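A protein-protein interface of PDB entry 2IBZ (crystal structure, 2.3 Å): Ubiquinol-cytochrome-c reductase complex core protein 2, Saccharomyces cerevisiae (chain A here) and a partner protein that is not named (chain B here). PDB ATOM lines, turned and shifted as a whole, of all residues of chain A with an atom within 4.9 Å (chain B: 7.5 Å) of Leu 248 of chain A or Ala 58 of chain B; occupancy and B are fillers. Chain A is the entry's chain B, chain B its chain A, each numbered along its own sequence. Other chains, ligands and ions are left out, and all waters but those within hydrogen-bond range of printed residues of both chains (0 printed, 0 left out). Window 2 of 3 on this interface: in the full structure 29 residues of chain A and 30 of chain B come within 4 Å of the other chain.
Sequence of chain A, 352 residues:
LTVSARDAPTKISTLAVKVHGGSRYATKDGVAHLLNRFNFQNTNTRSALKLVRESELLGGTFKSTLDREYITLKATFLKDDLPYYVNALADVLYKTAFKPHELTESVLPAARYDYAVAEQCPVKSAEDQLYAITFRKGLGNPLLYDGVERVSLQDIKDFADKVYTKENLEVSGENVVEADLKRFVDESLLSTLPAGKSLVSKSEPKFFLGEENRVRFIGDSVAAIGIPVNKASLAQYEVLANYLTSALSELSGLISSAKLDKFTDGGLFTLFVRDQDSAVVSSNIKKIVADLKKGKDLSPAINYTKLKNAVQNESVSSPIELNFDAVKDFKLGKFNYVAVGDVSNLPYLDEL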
ATOM      1  N   TYR A 243     -34.569 -13.787  22.408  1.00  0.00           N
ATOM      2  CA  TYR A 243     -34.256 -13.998  20.997  1.00  0.00           C
ATOM      3  C   TYR A 243     -35.506 -13.630  20.204  1.00  0.00           C
ATOM      4  O   TYR A 243     -35.441 -12.839  19.261  1.00  0.00           O
ATOM      5  CB  TYR A 243     -33.860 -15.466  20.753  1.00  0.00           C
ATOM      6  CG  TYR A 243     -33.812 -15.903  19.300  1.00  0.00           C
ATOM      7  CD1 TYR A 243     -32.836 -15.415  18.426  1.00  0.00           C
ATOM      8  CD2 TYR A 243     -34.752 -16.810  18.798  1.00  0.00           C
ATOM      9  CE1 TYR A 243     -32.800 -15.821  17.084  1.00  0.00           C
ATOM     10  CE2 TYR A 243     -34.726 -17.221  17.465  1.00  0.00           C
ATOM     11  CZ  TYR A 243     -33.752 -16.723  16.614  1.00  0.00           C
ATOM     12  OH  TYR A 243     -33.752 -17.119  15.294  1.00  0.00           O
ATOM     13  N   SER A 246     -36.263  -9.752  19.790  1.00  0.00           N
ATOM     14  CA  SER A 246     -35.089  -9.016  19.333  1.00  0.00           C
ATOM     15  C   SER A 246     -35.000  -8.967  17.813  1.00  0.00           C
ATOM     16  O   SER A 246     -35.691  -9.713  17.111  1.00  0.00           O
ATOM     17  CB  SER A 246     -33.809  -9.619  19.918  1.00  0.00           C
ATOM     18  OG  SER A 246     -33.701 -10.994  19.612  1.00  0.00           O
ATOM     19  N   ALA A 247     -34.141  -8.081  17.314  1.00  0.00           N
ATOM     20  CA  ALA A 247     -33.950  -7.904  15.878  1.00  0.00           C
ATOM     21  C   ALA A 247     -33.269  -9.099  15.203  1.00  0.00           C
ATOM     22  O   ALA A 247     -33.208  -9.178  13.971  1.00  0.00           O
ATOM     23  CB  ALA A 247     -33.174  -6.632  15.616  1.00  0.00           C
ATOM     24  N   LEU A 248     -32.770 -10.029  16.017  1.00  0.00           N
ATOM     25  CA  LEU A 248     -32.101 -11.226  15.515  1.00  0.00           C
ATOM     26  C   LEU A 248     -33.109 -12.187  14.904  1.00  0.00           C
ATOM     27  O   LEU A 248     -32.878 -12.730  13.824  1.00  0.00           O
ATOM     28  CB  LEU A 248     -31.331 -11.913  16.643  1.00  0.00           C
ATOM     29  CG  LEU A 248     -30.278 -11.027  17.311  1.00  0.00           C
ATOM     30  CD1 LEU A 248     -29.616 -11.767  18.451  1.00  0.00           C
ATOM     31  CD2 LEU A 248     -29.250 -10.584  16.290  1.00  0.00           C
ATOM     32  N   SER A 249     -34.227 -12.390  15.591  1.00  0.00           N
ATOM     33  CA  SER A 249     -35.269 -13.273  15.091  1.00  0.00           C
ATOM     34  C   SER A 249     -36.088 -12.558  14.030  1.00  0.00           C
ATOM     35  O   SER A 249     -36.442 -11.388  14.187  1.00  0.00           O
ATOM     36  CB  SER A 249     -36.186 -13.731  16.218  1.00  0.00           C
ATOM     37  OG  SER A 249     -37.221 -14.547  15.702  1.00  0.00           O
ATOM     38  N   GLU A 250     -36.370 -13.264  12.941  1.00  0.00           N
ATOM     39  CA  GLU A 250     -37.150 -12.698  11.849  1.00  0.00           C
ATOM     40  C   GLU A 250     -38.601 -12.594  12.281  1.00  0.00           C
ATOM     41  O   GLU A 250     -39.287 -11.614  11.973  1.00  0.00           O
ATOM     42  CB  GLU A 250     -37.050 -13.576  10.600  1.00  0.00           C
ATOM     43  CG  GLU A 250     -35.646 -13.708  10.022  1.00  0.00           C
ATOM     44  CD  GLU A 250     -35.626 -14.440   8.685  1.00  0.00           C
ATOM     45  OE1 GLU A 250     -36.332 -15.469   8.548  1.00  0.00           O
ATOM     46  OE2 GLU A 250     -34.907 -13.979   7.769  1.00  0.00           O
ATOM     47  N   PRO A 300     -26.591 -16.841  19.035  1.00  0.00           N
ATOM     48  CA  PRO A 300     -26.001 -15.561  18.628  1.00  0.00           C
ATOM     49  C   PRO A 300     -26.411 -14.483  19.631  1.00  0.00           C
ATOM     50  O   PRO A 300     -25.713 -13.482  19.815  1.00  0.00           O
ATOM     51  CB  PRO A 300     -26.652 -15.301  17.263  1.00  0.00           C
ATOM     52  CG  PRO A 300     -27.196 -16.653  16.838  1.00  0.00           C
ATOM     53  CD  PRO A 300     -27.693 -17.202  18.133  1.00  0.00           C
ATOM     54  N   ALA A 301     -27.551 -14.721  20.279  1.00  0.00           N
ATOM     55  CA  ALA A 301     -28.123 -13.817  21.272  1.00  0.00           C
ATOM     56  C   ALA A 301     -27.617 -14.106  22.681  1.00  0.00           C
ATOM     57  O   ALA A 301     -28.264 -13.745  23.661  1.00  0.00           O
ATOM     58  CB  ALA A 301     -29.647 -13.911  21.237  1.00  0.00           C
ATOM     59  N   LEU B  52     -33.483   2.609  15.202  1.00  0.00           N
ATOM     60  CA  LEU B  52     -33.948   1.412  15.896  1.00  0.00           C
ATOM     61  C   LEU B  52     -34.508   0.392  14.903  1.00  0.00           C
ATOM     62  O   LEU B  52     -35.202  -0.551  15.294  1.00  0.00           O
ATOM     63  CB  LEU B  52     -35.021   1.769  16.935  1.00  0.00           C
ATOM     64  CG  LEU B  52     -34.678   2.736  18.075  1.00  0.00           C
ATOM     65  CD1 LEU B  52     -35.894   2.935  18.962  1.00  0.00           C
ATOM     66  CD2 LEU B  52     -33.528   2.200  18.892  1.00  0.00           C
ATOM     67  N   SER B  53     -34.206   0.591  13.622  1.00  0.00           N
ATOM     68  CA  SER B  53     -34.664  -0.299  12.557  1.00  0.00           C
ATOM     69  C   SER B  53     -34.221  -1.733  12.790  1.00  0.00           C
ATOM     70  O   SER B  53     -33.202  -1.969  13.432  1.00  0.00           O
ATOM     71  CB  SER B  53     -34.120   0.173  11.210  1.00  0.00           C
ATOM     72  OG  SER B  53     -34.258  -0.832  10.220  1.00  0.00           O
ATOM     73  N   LYS B  54     -34.966  -2.682  12.227  1.00  0.00           N
ATOM     74  CA  LYS B  54     -34.647  -4.099  12.373  1.00  0.00           C
ATOM     75  C   LYS B  54     -33.210  -4.397  11.942  1.00  0.00           C
ATOM     76  O   LYS B  54     -32.513  -5.181  12.588  1.00  0.00           O
ATOM     77  CB  LYS B  54     -35.635  -4.963  11.578  1.00  0.00           C
ATOM     78  CG  LYS B  54     -35.358  -6.461  11.668  1.00  0.00           C
ATOM     79  CD  LYS B  54     -36.456  -7.303  11.023  1.00  0.00           C
ATOM     80  CE  LYS B  54     -37.730  -7.306  11.865  1.00  0.00           C
ATOM     81  NZ  LYS B  54     -38.742  -8.288  11.369  1.00  0.00           N
ATOM     82  N   GLU B  55     -32.764  -3.734  10.878  1.00  0.00           N
ATOM     83  CA  GLU B  55     -31.411  -3.922  10.366  1.00  0.00           C
ATOM     84  C   GLU B  55     -30.340  -3.404  11.318  1.00  0.00           C
ATOM     85  O   GLU B  55     -29.445  -4.148  11.712  1.00  0.00           O
ATOM     86  CB  GLU B  55     -31.241  -3.246   9.005  1.00  0.00           C
ATOM     87  CG  GLU B  55     -31.994  -3.909   7.865  1.00  0.00           C
ATOM     88  CD  GLU B  55     -31.594  -3.349   6.510  1.00  0.00           C
ATOM     89  OE1 GLU B  55     -31.860  -2.154   6.246  1.00  0.00           O
ATOM     90  OE2 GLU B  55     -31.000  -4.107   5.712  1.00  0.00           O
ATOM     91  N   ASN B  56     -30.429  -2.130  11.682  1.00  0.00           N
ATOM     92  CA  ASN B  56     -29.450  -1.523  12.576  1.00  0.00           C
ATOM     93  C   ASN B  56     -29.499  -2.137  13.970  1.00  0.00           C
ATOM     94  O   ASN B  56     -28.477  -2.238  14.647  1.00  0.00           O
ATOM     95  CB  ASN B  56     -29.683  -0.014  12.663  1.00  0.00           C
ATOM     96  CG  ASN B  56     -28.524   0.721  13.311  1.00  0.00           C
ATOM     97  OD1 ASN B  56     -27.398   0.686  12.817  1.00  0.00           O
ATOM     98  ND2 ASN B  56     -28.797   1.402  14.414  1.00  0.00           N
ATOM     99  N   SER B  57     -30.684  -2.573  14.383  1.00  0.00           N
ATOM    100  CA  SER B  57     -30.865  -3.162  15.703  1.00  0.00           C
ATOM    101  C   SER B  57     -30.292  -4.575  15.802  1.00  0.00           C
ATOM    102  O   SER B  57     -29.788  -4.965  16.854  1.00  0.00           O
ATOM    103  CB  SER B  57     -32.348  -3.148  16.098  1.00  0.00           C
ATOM    104  OG  SER B  57     -32.515  -3.309  17.496  1.00  0.00           O
ATOM    105  N   ALA B  58     -30.369  -5.335  14.711  1.00  0.00           N
ATOM    106  CA  ALA B  58     -29.843  -6.702  14.681  1.00  0.00           C
ATOM    107  C   ALA B  58     -28.316  -6.710  14.744  1.00  0.00           C
ATOM    108  O   ALA B  58     -27.716  -7.608  15.342  1.00  0.00           O
ATOM    109  CB  ALA B  58     -30.323  -7.432  13.432  1.00  0.00           C
ATOM    110  N   VAL B  59     -27.699  -5.702  14.128  1.00  0.00           N
ATOM    111  CA  VAL B  59     -26.246  -5.566  14.115  1.00  0.00           C
ATOM    112  C   VAL B  59     -25.737  -5.353  15.536  1.00  0.00           C
ATOM    113  O   VAL B  59     -24.681  -5.864  15.903  1.00  0.00           O
ATOM    114  CB  VAL B  59     -25.793  -4.389  13.209  1.00  0.00           C
ATOM    115  CG1 VAL B  59     -24.292  -4.159  13.328  1.00  0.00           C
ATOM    116  CG2 VAL B  59     -26.155  -4.676  11.762  1.00  0.00           C
ATOM    117  N   ALA B  60     -26.507  -4.618  16.337  1.00  0.00           N
ATOM    118  CA  ALA B  60     -26.141  -4.346  17.726  1.00  0.00           C
ATOM    119  C   ALA B  60     -26.489  -5.507  18.657  1.00  0.00           C
ATOM    120  O   ALA B  60     -25.855  -5.682  19.695  1.00  0.00           O
ATOM    121  CB  ALA B  60     -26.810  -3.071  18.210  1.00  0.00           C
ATOM    122  N   ALA B  61     -27.495  -6.294  18.282  1.00  0.00           N
ATOM    123  CA  ALA B  61     -27.931  -7.436  19.082  1.00  0.00           C
ATOM    124  C   ALA B  61     -26.933  -8.588  19.024  1.00  0.00           C
ATOM    125  O   ALA B  61     -26.768  -9.322  20.001  1.00  0.00           O
ATOM    126  CB  ALA B  61     -29.302  -7.898  18.632  1.00  0.00           C
ATOM    127  N   LYS B  62     -26.288  -8.756  17.869  1.00  0.00           N
ATOM    128  CA  LYS B  62     -25.277  -9.800  17.688  1.00  0.00           C
ATOM    129  C   LYS B  62     -24.118  -9.470  18.624  1.00  0.00           C
ATOM    130  O   LYS B  62     -23.609 -10.335  19.340  1.00  0.00           O
ATOM    131  CB  LYS B  62     -24.759  -9.806  16.243  1.00  0.00           C
ATOM    132  CG  LYS B  62     -25.717 -10.365  15.194  1.00  0.00           C
ATOM    133  CD  LYS B  62     -25.818 -11.887  15.263  1.00  0.00           C
ATOM    134  CE  LYS B  62     -26.679 -12.437  14.127  1.00  0.00           C
ATOM    135  NZ  LYS B  62     -26.794 -13.924  14.163  1.00  0.00           N
ATOM    136  N   GLU B  63     -23.747  -8.192  18.627  1.00  0.00           N
ATOM    137  CA  GLU B  63     -22.659  -7.666  19.442  1.00  0.00           C
ATOM    138  C   GLU B  63     -23.031  -7.577  20.930  1.00  0.00           C
ATOM    139  O   GLU B  63     -22.178  -7.284  21.772  1.00  0.00           O
ATOM    140  CB  GLU B  63     -22.256  -6.282  18.917  1.00  0.00           C
ATOM    141  CG  GLU B  63     -20.838  -5.848  19.268  1.00  0.00           C
ATOM    142  CD  GLU B  63     -19.776  -6.573  18.453  1.00  0.00           C
ATOM    143  OE1 GLU B  63     -19.333  -6.012  17.429  1.00  0.00           O
ATOM    144  OE2 GLU B  63     -19.378  -7.695  18.841  1.00  0.00           O
ATOM    145  N   GLY B  64     -24.301  -7.829  21.243  1.00  0.00           N
ATOM    146  CA  GLY B  64     -24.762  -7.775  22.624  1.00  0.00           C
ATOM    147  C   GLY B  64     -25.076  -6.382  23.148  1.00  0.00           C
ATOM    148  O   GLY B  64     -24.985  -6.128  24.354  1.00  0.00           O
ATOM    149  N   LEU B  65     -25.434  -5.479  22.239  1.00  0.00           N
ATOM    150  CA  LEU B  65     -25.774  -4.098  22.577  1.00  0.00           C
ATOM    151  C   LEU B  65     -27.278  -3.840  22.406  1.00  0.00           C
ATOM    152  O   LEU B  65     -27.910  -4.401  21.509  1.00  0.00           O
ATOM    153  CB  LEU B  65     -24.975  -3.133  21.693  1.00  0.00           C
ATOM    154  CG  LEU B  65     -23.528  -2.796  22.075  1.00  0.00           C
ATOM    155  CD1 LEU B  65     -22.708  -4.047  22.301  1.00  0.00           C
ATOM    156  CD2 LEU B  65     -22.907  -1.939  20.990  1.00  0.00           C
ATOM    157  N   LEU B  67     -30.368  -0.947  21.917  1.00  0.00           N
ATOM    158  CA  LEU B  67     -30.610   0.412  21.438  1.00  0.00           C
ATOM    159  C   LEU B  67     -31.798   1.124  22.076  1.00  0.00           C
ATOM    160  O   LEU B  67     -32.807   0.501  22.413  1.00  0.00           O
ATOM    161  CB  LEU B  67     -30.769   0.402  19.917  1.00  0.00           C
ATOM    162  CG  LEU B  67     -29.632  -0.249  19.128  1.00  0.00           C
ATOM    163  CD1 LEU B  67     -29.902  -0.130  17.640  1.00  0.00           C
ATOM    164  CD2 LEU B  67     -28.311   0.402  19.493  1.00  0.00           C
ATOM    165  N   PHE B  93     -20.233   1.061  17.415  1.00  0.00           N
ATOM    166  CA  PHE B  93     -21.577   1.033  16.856  1.00  0.00           C
ATOM    167  C   PHE B  93     -22.161   2.438  16.722  1.00  0.00           C
ATOM    168  O   PHE B  93     -22.997   2.690  15.855  1.00  0.00           O
ATOM    169  CB  PHE B  93     -22.492   0.162  17.720  1.00  0.00           C
ATOM    170  CG  PHE B  93     -23.809  -0.144  17.075  1.00  0.00           C
ATOM    171  CD1 PHE B  93     -23.918  -1.176  16.151  1.00  0.00           C
ATOM    172  CD2 PHE B  93     -24.931   0.626  17.355  1.00  0.00           C
ATOM    173  CE1 PHE B  93     -25.125  -1.434  15.511  1.00  0.00           C
ATOM    174  CE2 PHE B  93     -26.142   0.374  16.719  1.00  0.00           C
ATOM    175  CZ  PHE B  93     -26.237  -0.657  15.794  1.00  0.00           C
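Among the printed residues, merely in contact across the chains: Ala 247 of chain A with Ala 58 of chain B, Pro 300 of chain A with Lys 62 of chain B, Ala 247 of chain A with Lys 54 of chain B, Leu 248 of chain A with Ala 58 of chain B, Leu 248 of chain A with Ala 61 of chain B, Ala 247 of chain A with Ser 57 of chain B and Leu 248 of chain A with Lys 62 of chain B.
The side-chain amino group (NZ) of Lys 54 of chain B is in hydrogen-bond range of the backbone carbonyl oxygen (O) of Glu 250 of chain A, at 3.4 Å.
Of the printed residues of chain B, Leu 248 of chain A touches Ala 58, Ala 61 and Lys 62. Ala 58 of chain B touches just these residues of chain A: Ala 247 (3.2 Å) and Leu 248 (3.5 Å). Of chain B, only Lys 54, Ser 57 and Ala 58 come within 4 Å of Ala 247 of chain A. Printed residues of chain A within 4 Å of Lys 62 of chain B: Leu 248 (3.7 Å) and Pro 300 (3.4 Å). Of the printed residues of chain A, Lys 54 of chain B touches Ala 247 (3.4 Å) and Glu 250 (3.4 Å). Printed residues of chain B within 4 Å of Glu 250 of chain A: Lys 54 (3.4 Å). The nearest residue of chain B that does not touch Leu 248 of chain A is Val 59 of chain B (5.6 Å). The nearest printed residue of chain A that does not touch Ala 58 of chain B is Ser 246 of chain A (6.4 Å). The nearest printed residue of chain A that does not touch Lys 54 of chain B is Ser 249 of chain A (4.8 Å).
Of the 16 printed residues of chain B, 5 touch a printed residue of chain A. Hydrophobic or aromatic side chains of chain B that line the printed part of chain A: Ala 58 and Ala 61. Along chain B the printed residues that touch a printed residue of chain A span positions 54 to 62. Of the 8 printed residues of chain A, 4 touch a printed residue of chain B. Hydrophobic or aromatic side chains of chain A that line the printed part of chain B: Ala 247, Leu 248 and Pro 300. Among the printed residues, no Asp or Glu carboxylate lies within 4 Å of a Lys or Arg side-chain nitrogen of the other chain.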
